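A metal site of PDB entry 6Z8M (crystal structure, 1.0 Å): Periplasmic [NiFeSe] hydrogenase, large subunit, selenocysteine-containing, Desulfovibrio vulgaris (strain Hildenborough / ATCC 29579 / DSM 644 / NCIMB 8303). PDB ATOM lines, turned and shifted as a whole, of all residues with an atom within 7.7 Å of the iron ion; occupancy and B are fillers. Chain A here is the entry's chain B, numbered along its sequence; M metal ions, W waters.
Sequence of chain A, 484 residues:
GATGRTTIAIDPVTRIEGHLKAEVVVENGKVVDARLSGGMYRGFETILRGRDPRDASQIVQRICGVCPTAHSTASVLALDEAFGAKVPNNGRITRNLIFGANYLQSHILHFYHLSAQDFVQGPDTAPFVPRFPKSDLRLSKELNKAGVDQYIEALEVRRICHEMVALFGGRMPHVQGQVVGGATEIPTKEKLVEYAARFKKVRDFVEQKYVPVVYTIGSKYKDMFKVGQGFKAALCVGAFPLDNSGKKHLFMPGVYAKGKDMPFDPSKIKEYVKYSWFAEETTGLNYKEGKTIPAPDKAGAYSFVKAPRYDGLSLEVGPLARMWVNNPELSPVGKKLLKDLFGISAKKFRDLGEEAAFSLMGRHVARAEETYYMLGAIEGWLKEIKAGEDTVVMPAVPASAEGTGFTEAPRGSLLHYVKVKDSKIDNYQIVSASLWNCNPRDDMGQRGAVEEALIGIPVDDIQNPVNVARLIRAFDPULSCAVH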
ATOM      1  N   GLU A  45      -8.041  -8.704  -5.899  1.00  0.00           N
ATOM      2  CA  GLU A  45      -6.840  -7.890  -5.806  1.00  0.00           C
ATOM      3  C   GLU A  45      -6.282  -7.508  -7.182  1.00  0.00           C
ATOM      4  O   GLU A  45      -5.537  -6.528  -7.283  1.00  0.00           O
ATOM      5  CB  GLU A  45      -5.788  -8.619  -4.972  1.00  0.00           C
ATOM      6  CG  GLU A  45      -6.197  -8.713  -3.507  1.00  0.00           C
ATOM      7  CD  GLU A  45      -5.636  -9.929  -2.749  1.00  0.00           C
ATOM      8  OE1 GLU A  45      -5.325 -10.946  -3.403  1.00  0.00           O
ATOM      9  OE2 GLU A  45      -5.549  -9.852  -1.491  1.00  0.00           O
ATOM     10  N   GLU A 271       2.513 -13.497   3.960  1.00  0.00           N
ATOM     11  CA  GLU A 271       1.652 -14.492   3.326  1.00  0.00           C
ATOM     12  C   GLU A 271       2.496 -15.448   2.491  1.00  0.00           C
ATOM     13  O   GLU A 271       3.167 -15.035   1.553  1.00  0.00           O
ATOM     14  CB  GLU A 271       0.548 -13.849   2.490  1.00  0.00           C
ATOM     15  CG  GLU A 271      -0.433 -13.050   3.325  1.00  0.00           C
ATOM     16  CD  GLU A 271      -1.623 -12.608   2.508  1.00  0.00           C
ATOM     17  OE1 GLU A 271      -1.494 -11.600   1.783  1.00  0.00           O
ATOM     18  OE2 GLU A 271      -2.657 -13.319   2.548  1.00  0.00           O
ATOM     19  N   PHE A 278      -0.741 -20.126  -6.135  1.00  0.00           N
ATOM     20  CA  PHE A 278      -0.153 -18.864  -6.574  1.00  0.00           C
ATOM     21  C   PHE A 278       1.302 -19.065  -6.935  1.00  0.00           C
ATOM     22  O   PHE A 278       1.959 -20.005  -6.474  1.00  0.00           O
ATOM     23  CB  PHE A 278      -0.306 -17.795  -5.488  1.00  0.00           C
ATOM     24  CG  PHE A 278      -1.726 -17.542  -5.135  1.00  0.00           C
ATOM     25  CD1 PHE A 278      -2.503 -16.750  -5.944  1.00  0.00           C
ATOM     26  CD2 PHE A 278      -2.325 -18.167  -4.065  1.00  0.00           C
ATOM     27  CE1 PHE A 278      -3.834 -16.562  -5.688  1.00  0.00           C
ATOM     28  CE2 PHE A 278      -3.665 -17.981  -3.799  1.00  0.00           C
ATOM     29  CZ  PHE A 278      -4.412 -17.179  -4.609  1.00  0.00           C
ATOM     30  N   TYR A 287       1.784  -7.658   3.286  1.00  0.00           N
ATOM     31  CA  TYR A 287       0.678  -7.182   2.452  1.00  0.00           C
ATOM     32  C   TYR A 287       1.006  -5.872   1.749  1.00  0.00           C
ATOM     33  O   TYR A 287       0.462  -5.598   0.677  1.00  0.00           O
ATOM     34  CB  TYR A 287      -0.621  -7.072   3.268  1.00  0.00           C
ATOM     35  CG  TYR A 287      -0.473  -6.172   4.463  1.00  0.00           C
ATOM     36  CD1 TYR A 287      -0.601  -4.804   4.332  1.00  0.00           C
ATOM     37  CD2 TYR A 287      -0.122  -6.682   5.702  1.00  0.00           C
ATOM     38  CE1 TYR A 287      -0.395  -3.954   5.399  1.00  0.00           C
ATOM     39  CE2 TYR A 287       0.089  -5.852   6.778  1.00  0.00           C
ATOM     40  CZ  TYR A 287      -0.037  -4.492   6.629  1.00  0.00           C
ATOM     41  OH  TYR A 287       0.179  -3.669   7.708  1.00  0.00           O
ATOM     42  N   LYS A 291       1.295  -9.645  -3.666  1.00  0.00           N
ATOM     43  CA  LYS A 291       1.085  -9.962  -5.074  1.00  0.00           C
ATOM     44  C   LYS A 291       0.132 -11.143  -5.155  1.00  0.00           C
ATOM     45  O   LYS A 291       0.172 -12.056  -4.316  1.00  0.00           O
ATOM     46  CB  LYS A 291       2.379 -10.357  -5.778  1.00  0.00           C
ATOM     47  CG  LYS A 291       3.378  -9.228  -5.835  1.00  0.00           C
ATOM     48  CD  LYS A 291       4.593  -9.605  -6.660  1.00  0.00           C
ATOM     49  CE  LYS A 291       5.392  -8.369  -7.086  1.00  0.00           C
ATOM     50  NZ  LYS A 291       4.575  -7.450  -7.936  1.00  0.00           N
ATOM     51  N   THR A 292      -0.699 -11.133  -6.185  1.00  0.00           N
ATOM     52  CA  THR A 292      -1.706 -12.171  -6.370  1.00  0.00           C
ATOM     53  C   THR A 292      -1.633 -12.642  -7.816  1.00  0.00           C
ATOM     54  O   THR A 292      -2.188 -12.010  -8.719  1.00  0.00           O
ATOM     55  CB  THR A 292      -3.067 -11.640  -5.972  1.00  0.00           C
ATOM     56  OG1 THR A 292      -2.946 -11.143  -4.641  1.00  0.00           O
ATOM     57  CG2 THR A 292      -4.109 -12.745  -6.024  1.00  0.00           C
ATOM     58  N   PHE A 304      -6.787 -22.124  -2.743  1.00  0.00           N
ATOM     59  CA  PHE A 304      -6.671 -20.741  -3.198  1.00  0.00           C
ATOM     60  C   PHE A 304      -6.518 -19.758  -2.047  1.00  0.00           C
ATOM     61  O   PHE A 304      -6.443 -18.542  -2.276  1.00  0.00           O
ATOM     62  CB  PHE A 304      -7.876 -20.346  -4.061  1.00  0.00           C
ATOM     63  CG  PHE A 304      -7.875 -20.955  -5.437  1.00  0.00           C
ATOM     64  CD1 PHE A 304      -6.911 -20.611  -6.370  1.00  0.00           C
ATOM     65  CD2 PHE A 304      -8.867 -21.849  -5.817  1.00  0.00           C
ATOM     66  CE1 PHE A 304      -6.915 -21.167  -7.648  1.00  0.00           C
ATOM     67  CE2 PHE A 304      -8.900 -22.398  -7.089  1.00  0.00           C
ATOM     68  CZ  PHE A 304      -7.911 -22.066  -8.005  1.00  0.00           C
ATOM     69  N   LYS A 306      -4.147 -18.113   0.641  1.00  0.00           N
ATOM     70  CA  LYS A 306      -2.741 -17.936   1.021  1.00  0.00           C
ATOM     71  C   LYS A 306      -2.569 -18.358   2.483  1.00  0.00           C
ATOM     72  O   LYS A 306      -3.549 -18.612   3.186  1.00  0.00           O
ATOM     73  CB  LYS A 306      -2.288 -16.490   0.813  1.00  0.00           C
ATOM     74  CG  LYS A 306      -2.313 -16.006  -0.632  1.00  0.00           C
ATOM     75  CD  LYS A 306      -1.844 -14.565  -0.730  1.00  0.00           C
ATOM     76  CE  LYS A 306      -1.844 -14.042  -2.166  1.00  0.00           C
ATOM     77  NZ  LYS A 306      -1.709 -12.548  -2.167  1.00  0.00           N
ATOM     78  N   LEU A 415      -7.755  -6.725   7.262  1.00  0.00           N
ATOM     79  CA  LEU A 415      -7.100  -5.500   6.831  1.00  0.00           C
ATOM     80  C   LEU A 415      -7.144  -5.421   5.320  1.00  0.00           C
ATOM     81  O   LEU A 415      -7.162  -6.435   4.611  1.00  0.00           O
ATOM     82  CB  LEU A 415      -5.679  -5.384   7.356  1.00  0.00           C
ATOM     83  CG  LEU A 415      -4.680  -6.369   6.779  1.00  0.00           C
ATOM     84  CD1 LEU A 415      -4.010  -5.810   5.525  1.00  0.00           C
ATOM     85  CD2 LEU A 415      -3.614  -6.768   7.796  1.00  0.00           C
ATOM     86  N   TYR A 428      -3.898  -3.440  -4.355  1.00  0.00           N
ATOM     87  CA  TYR A 428      -4.888  -3.555  -3.298  1.00  0.00           C
ATOM     88  C   TYR A 428      -4.724  -4.965  -2.749  1.00  0.00           C
ATOM     89  O   TYR A 428      -4.804  -5.927  -3.505  1.00  0.00           O
ATOM     90  CB  TYR A 428      -6.298  -3.318  -3.854  1.00  0.00           C
ATOM     91  CG  TYR A 428      -7.309  -2.926  -2.795  1.00  0.00           C
ATOM     92  CD1 TYR A 428      -7.814  -3.847  -1.882  1.00  0.00           C
ATOM     93  CD2 TYR A 428      -7.787  -1.621  -2.720  1.00  0.00           C
ATOM     94  CE1 TYR A 428      -8.744  -3.476  -0.928  1.00  0.00           C
ATOM     95  CE2 TYR A 428      -8.717  -1.249  -1.766  1.00  0.00           C
ATOM     96  CZ  TYR A 428      -9.196  -2.164  -0.886  1.00  0.00           C
ATOM     97  OH  TYR A 428     -10.136  -1.769   0.047  1.00  0.00           O
ATOM     98  N   GLN A 429      -4.452  -5.077  -1.458  1.00  0.00           N
ATOM     99  CA  GLN A 429      -4.241  -6.375  -0.842  1.00  0.00           C
ATOM    100  C   GLN A 429      -5.158  -6.549   0.350  1.00  0.00           C
ATOM    101  O   GLN A 429      -5.291  -5.636   1.176  1.00  0.00           O
ATOM    102  CB  GLN A 429      -2.773  -6.569  -0.450  1.00  0.00           C
ATOM    103  CG  GLN A 429      -1.870  -6.757  -1.651  1.00  0.00           C
ATOM    104  CD  GLN A 429      -2.087  -8.092  -2.333  1.00  0.00           C
ATOM    105  OE1 GLN A 429      -2.210  -9.113  -1.678  1.00  0.00           O
ATOM    106  NE2 GLN A 429      -2.075  -8.100  -3.655  1.00  0.00           N
ATOM    107  N   ILE A 430      -5.764  -7.720   0.440  1.00  0.00           N
ATOM    108  CA  ILE A 430      -6.737  -8.057   1.467  1.00  0.00           C
ATOM    109  C   ILE A 430      -6.205  -9.239   2.263  1.00  0.00           C
ATOM    110  O   ILE A 430      -5.796 -10.260   1.693  1.00  0.00           O
ATOM    111  CB  ILE A 430      -8.103  -8.383   0.836  1.00  0.00           C
ATOM    112  CG1 ILE A 430      -8.672  -7.098   0.212  1.00  0.00           C
ATOM    113  CG2 ILE A 430      -9.076  -8.920   1.878  1.00  0.00           C
ATOM    114  CD1 ILE A 430      -9.327  -7.322  -1.080  1.00  0.00           C
ATOM    115  N   VAL A 431      -6.226  -9.099   3.586  1.00  0.00           N
ATOM    116  CA  VAL A 431      -5.845 -10.154   4.515  1.00  0.00           C
ATOM    117  C   VAL A 431      -7.046 -10.275   5.463  1.00  0.00           C
ATOM    118  O   VAL A 431      -7.262  -9.401   6.298  1.00  0.00           O
ATOM    119  CB  VAL A 431      -4.548  -9.801   5.271  1.00  0.00           C
ATOM    120  CG1 VAL A 431      -4.162 -10.875   6.273  1.00  0.00           C
ATOM    121  CG2 VAL A 431      -3.401  -9.556   4.271  1.00  0.00           C
ATOM    122  N   SER A 432      -7.853 -11.323   5.285  1.00  0.00           N
ATOM    123  CA  SER A 432      -9.185 -11.423   5.882  1.00  0.00           C
ATOM    124  C   SER A 432      -9.261 -12.490   6.990  1.00  0.00           C
ATOM    125  O   SER A 432      -8.313 -13.235   7.252  1.00  0.00           O
ATOM    126  CB  SER A 432     -10.170 -11.792   4.786  1.00  0.00           C
ATOM    127  OG  SER A 432      -9.782 -13.044   4.264  1.00  0.00           O
ATOM    128  N   LEU A 435      -9.163 -16.192   6.018  1.00  0.00           N
ATOM    129  CA  LEU A 435      -7.792 -16.437   5.593  1.00  0.00           C
ATOM    130  C   LEU A 435      -6.948 -16.875   6.784  1.00  0.00           C
ATOM    131  O   LEU A 435      -6.215 -17.866   6.687  1.00  0.00           O
ATOM    132  CB  LEU A 435      -7.258 -15.169   4.933  1.00  0.00           C
ATOM    133  CG  LEU A 435      -5.746 -15.071   4.791  1.00  0.00           C
ATOM    134  CD1 LEU A 435      -5.221 -15.978   3.710  1.00  0.00           C
ATOM    135  CD2 LEU A 435      -5.351 -13.635   4.518  1.00  0.00           C
ATOM    136  N   CYS A 481     -14.471 -14.930   1.644  1.00  0.00           N
ATOM    137  CA  CYS A 481     -13.559 -13.983   2.290  1.00  0.00           C
ATOM    138  C   CYS A 481     -12.126 -14.481   2.261  1.00  0.00           C
ATOM    139  O   CYS A 481     -11.203 -13.690   2.053  1.00  0.00           O
ATOM    140  CB  CYS A 481     -13.930 -13.773   3.744  1.00  0.00           C
ATOM    141  SG  CYS A 481     -15.208 -12.561   3.996  1.00  0.00           S
ATOM    142  N   ALA A 482     -11.912 -15.769   2.528  1.00  0.00           N
ATOM    143  CA  ALA A 482     -10.556 -16.288   2.653  1.00  0.00           C
ATOM    144  C   ALA A 482      -9.782 -16.177   1.346  1.00  0.00           C
ATOM    145  O   ALA A 482      -8.584 -15.894   1.369  1.00  0.00           O
ATOM    146  CB  ALA A 482     -10.600 -17.752   3.101  1.00  0.00           C
ATOM    147  N   VAL A 483     -10.447 -16.392   0.211  1.00  0.00           N
ATOM    148  CA  VAL A 483      -9.801 -16.415  -1.094  1.00  0.00           C
ATOM    149  C   VAL A 483      -9.871 -15.080  -1.801  1.00  0.00           C
ATOM    150  O   VAL A 483      -8.890 -14.642  -2.404  1.00  0.00           O
ATOM    151  CB  VAL A 483     -10.404 -17.528  -1.976  1.00  0.00           C
ATOM    152  CG1 VAL A 483      -9.754 -17.490  -3.338  1.00  0.00           C
ATOM    153  CG2 VAL A 483     -10.240 -18.908  -1.331  1.00  0.00           C
ATOM    154  N   HIS A 484     -11.049 -14.471  -1.842  1.00  0.00           N
ATOM    155  CA  HIS A 484     -11.276 -13.234  -2.564  1.00  0.00           C
ATOM    156  C   HIS A 484     -10.721 -13.291  -3.991  1.00  0.00           C
ATOM    157  O   HIS A 484     -10.983 -14.297  -4.688  1.00  0.00           O
ATOM    158  CB  HIS A 484     -10.850 -11.975  -1.763  1.00  0.00           C
ATOM    159  CG  HIS A 484      -9.537 -12.080  -1.039  1.00  0.00           C
ATOM    160  ND1 HIS A 484      -9.416 -12.694   0.183  1.00  0.00           N
ATOM    161  CD2 HIS A 484      -8.300 -11.606  -1.338  1.00  0.00           C
ATOM    162  CE1 HIS A 484      -8.152 -12.622   0.596  1.00  0.00           C
ATOM    163  NE2 HIS A 484      -7.453 -11.983  -0.322  1.00  0.00           N
ATOM    164  OXT HIS A 484     -10.096 -12.326  -4.450  1.00  0.00           O
HETATM  165 FE    FE M   1      -5.321 -11.499  -0.090  1.00  0.00          FE
HETATM  166  O   HOH W   1      -4.938 -13.135   1.199  1.00  0.00           O
HETATM  167  O   HOH W   2      -4.836 -12.944  -1.769  1.00  0.00           O
HETATM  168  O   HOH W   3      -3.211 -10.945  -0.059  1.00  0.00           O
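The side-chain carboxylate (OE1) of Glu 45 is in hydrogen-bond range of the side-chain hydroxyl (OG1) of Thr 292, at 2.7 Å. The side-chain carboxylate (OE2) of Glu 45 sits close to the side-chain amide oxygen (OE1) of Gln 429 (3.4 Å). A ring nitrogen (ND1) of His 484 is in hydrogen-bond range of the backbone carbonyl oxygen (O) of Cys 481 (2.8 Å).
The nearest printed residue that does not touch the iron ion is Glu 271 (4.2 Å).
Water W1 is bound to the iron ion, at 2.1 Å. The side-chain carboxylate (OE2) of Glu 45 binds the iron ion, at 2.2 Å. Water W3 is bound to the iron ion, at 2.2 Å. NE2 of His 484 is bound to the iron ion, 2.2 Å away. The iron ion is bound by the backbone carbonyl oxygen (O) of Ile 430, at 2.2 Å. Water W2 binds the iron ion, at 2.3 Å.
Water W3 lies within hydrogen-bond range of the side-chain carboxylate (OE1) of Glu 271 (2.6 Å), the side-chain amide oxygen (OE1) of Gln 429 (2.6 Å) and the side-chain amino group (NZ) of Lys 306 (3.0 Å). Water W2 lies within hydrogen-bond range of OE1 of Glu 45 (2.6 Å) and NZ of Lys 306 (3.2 Å).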
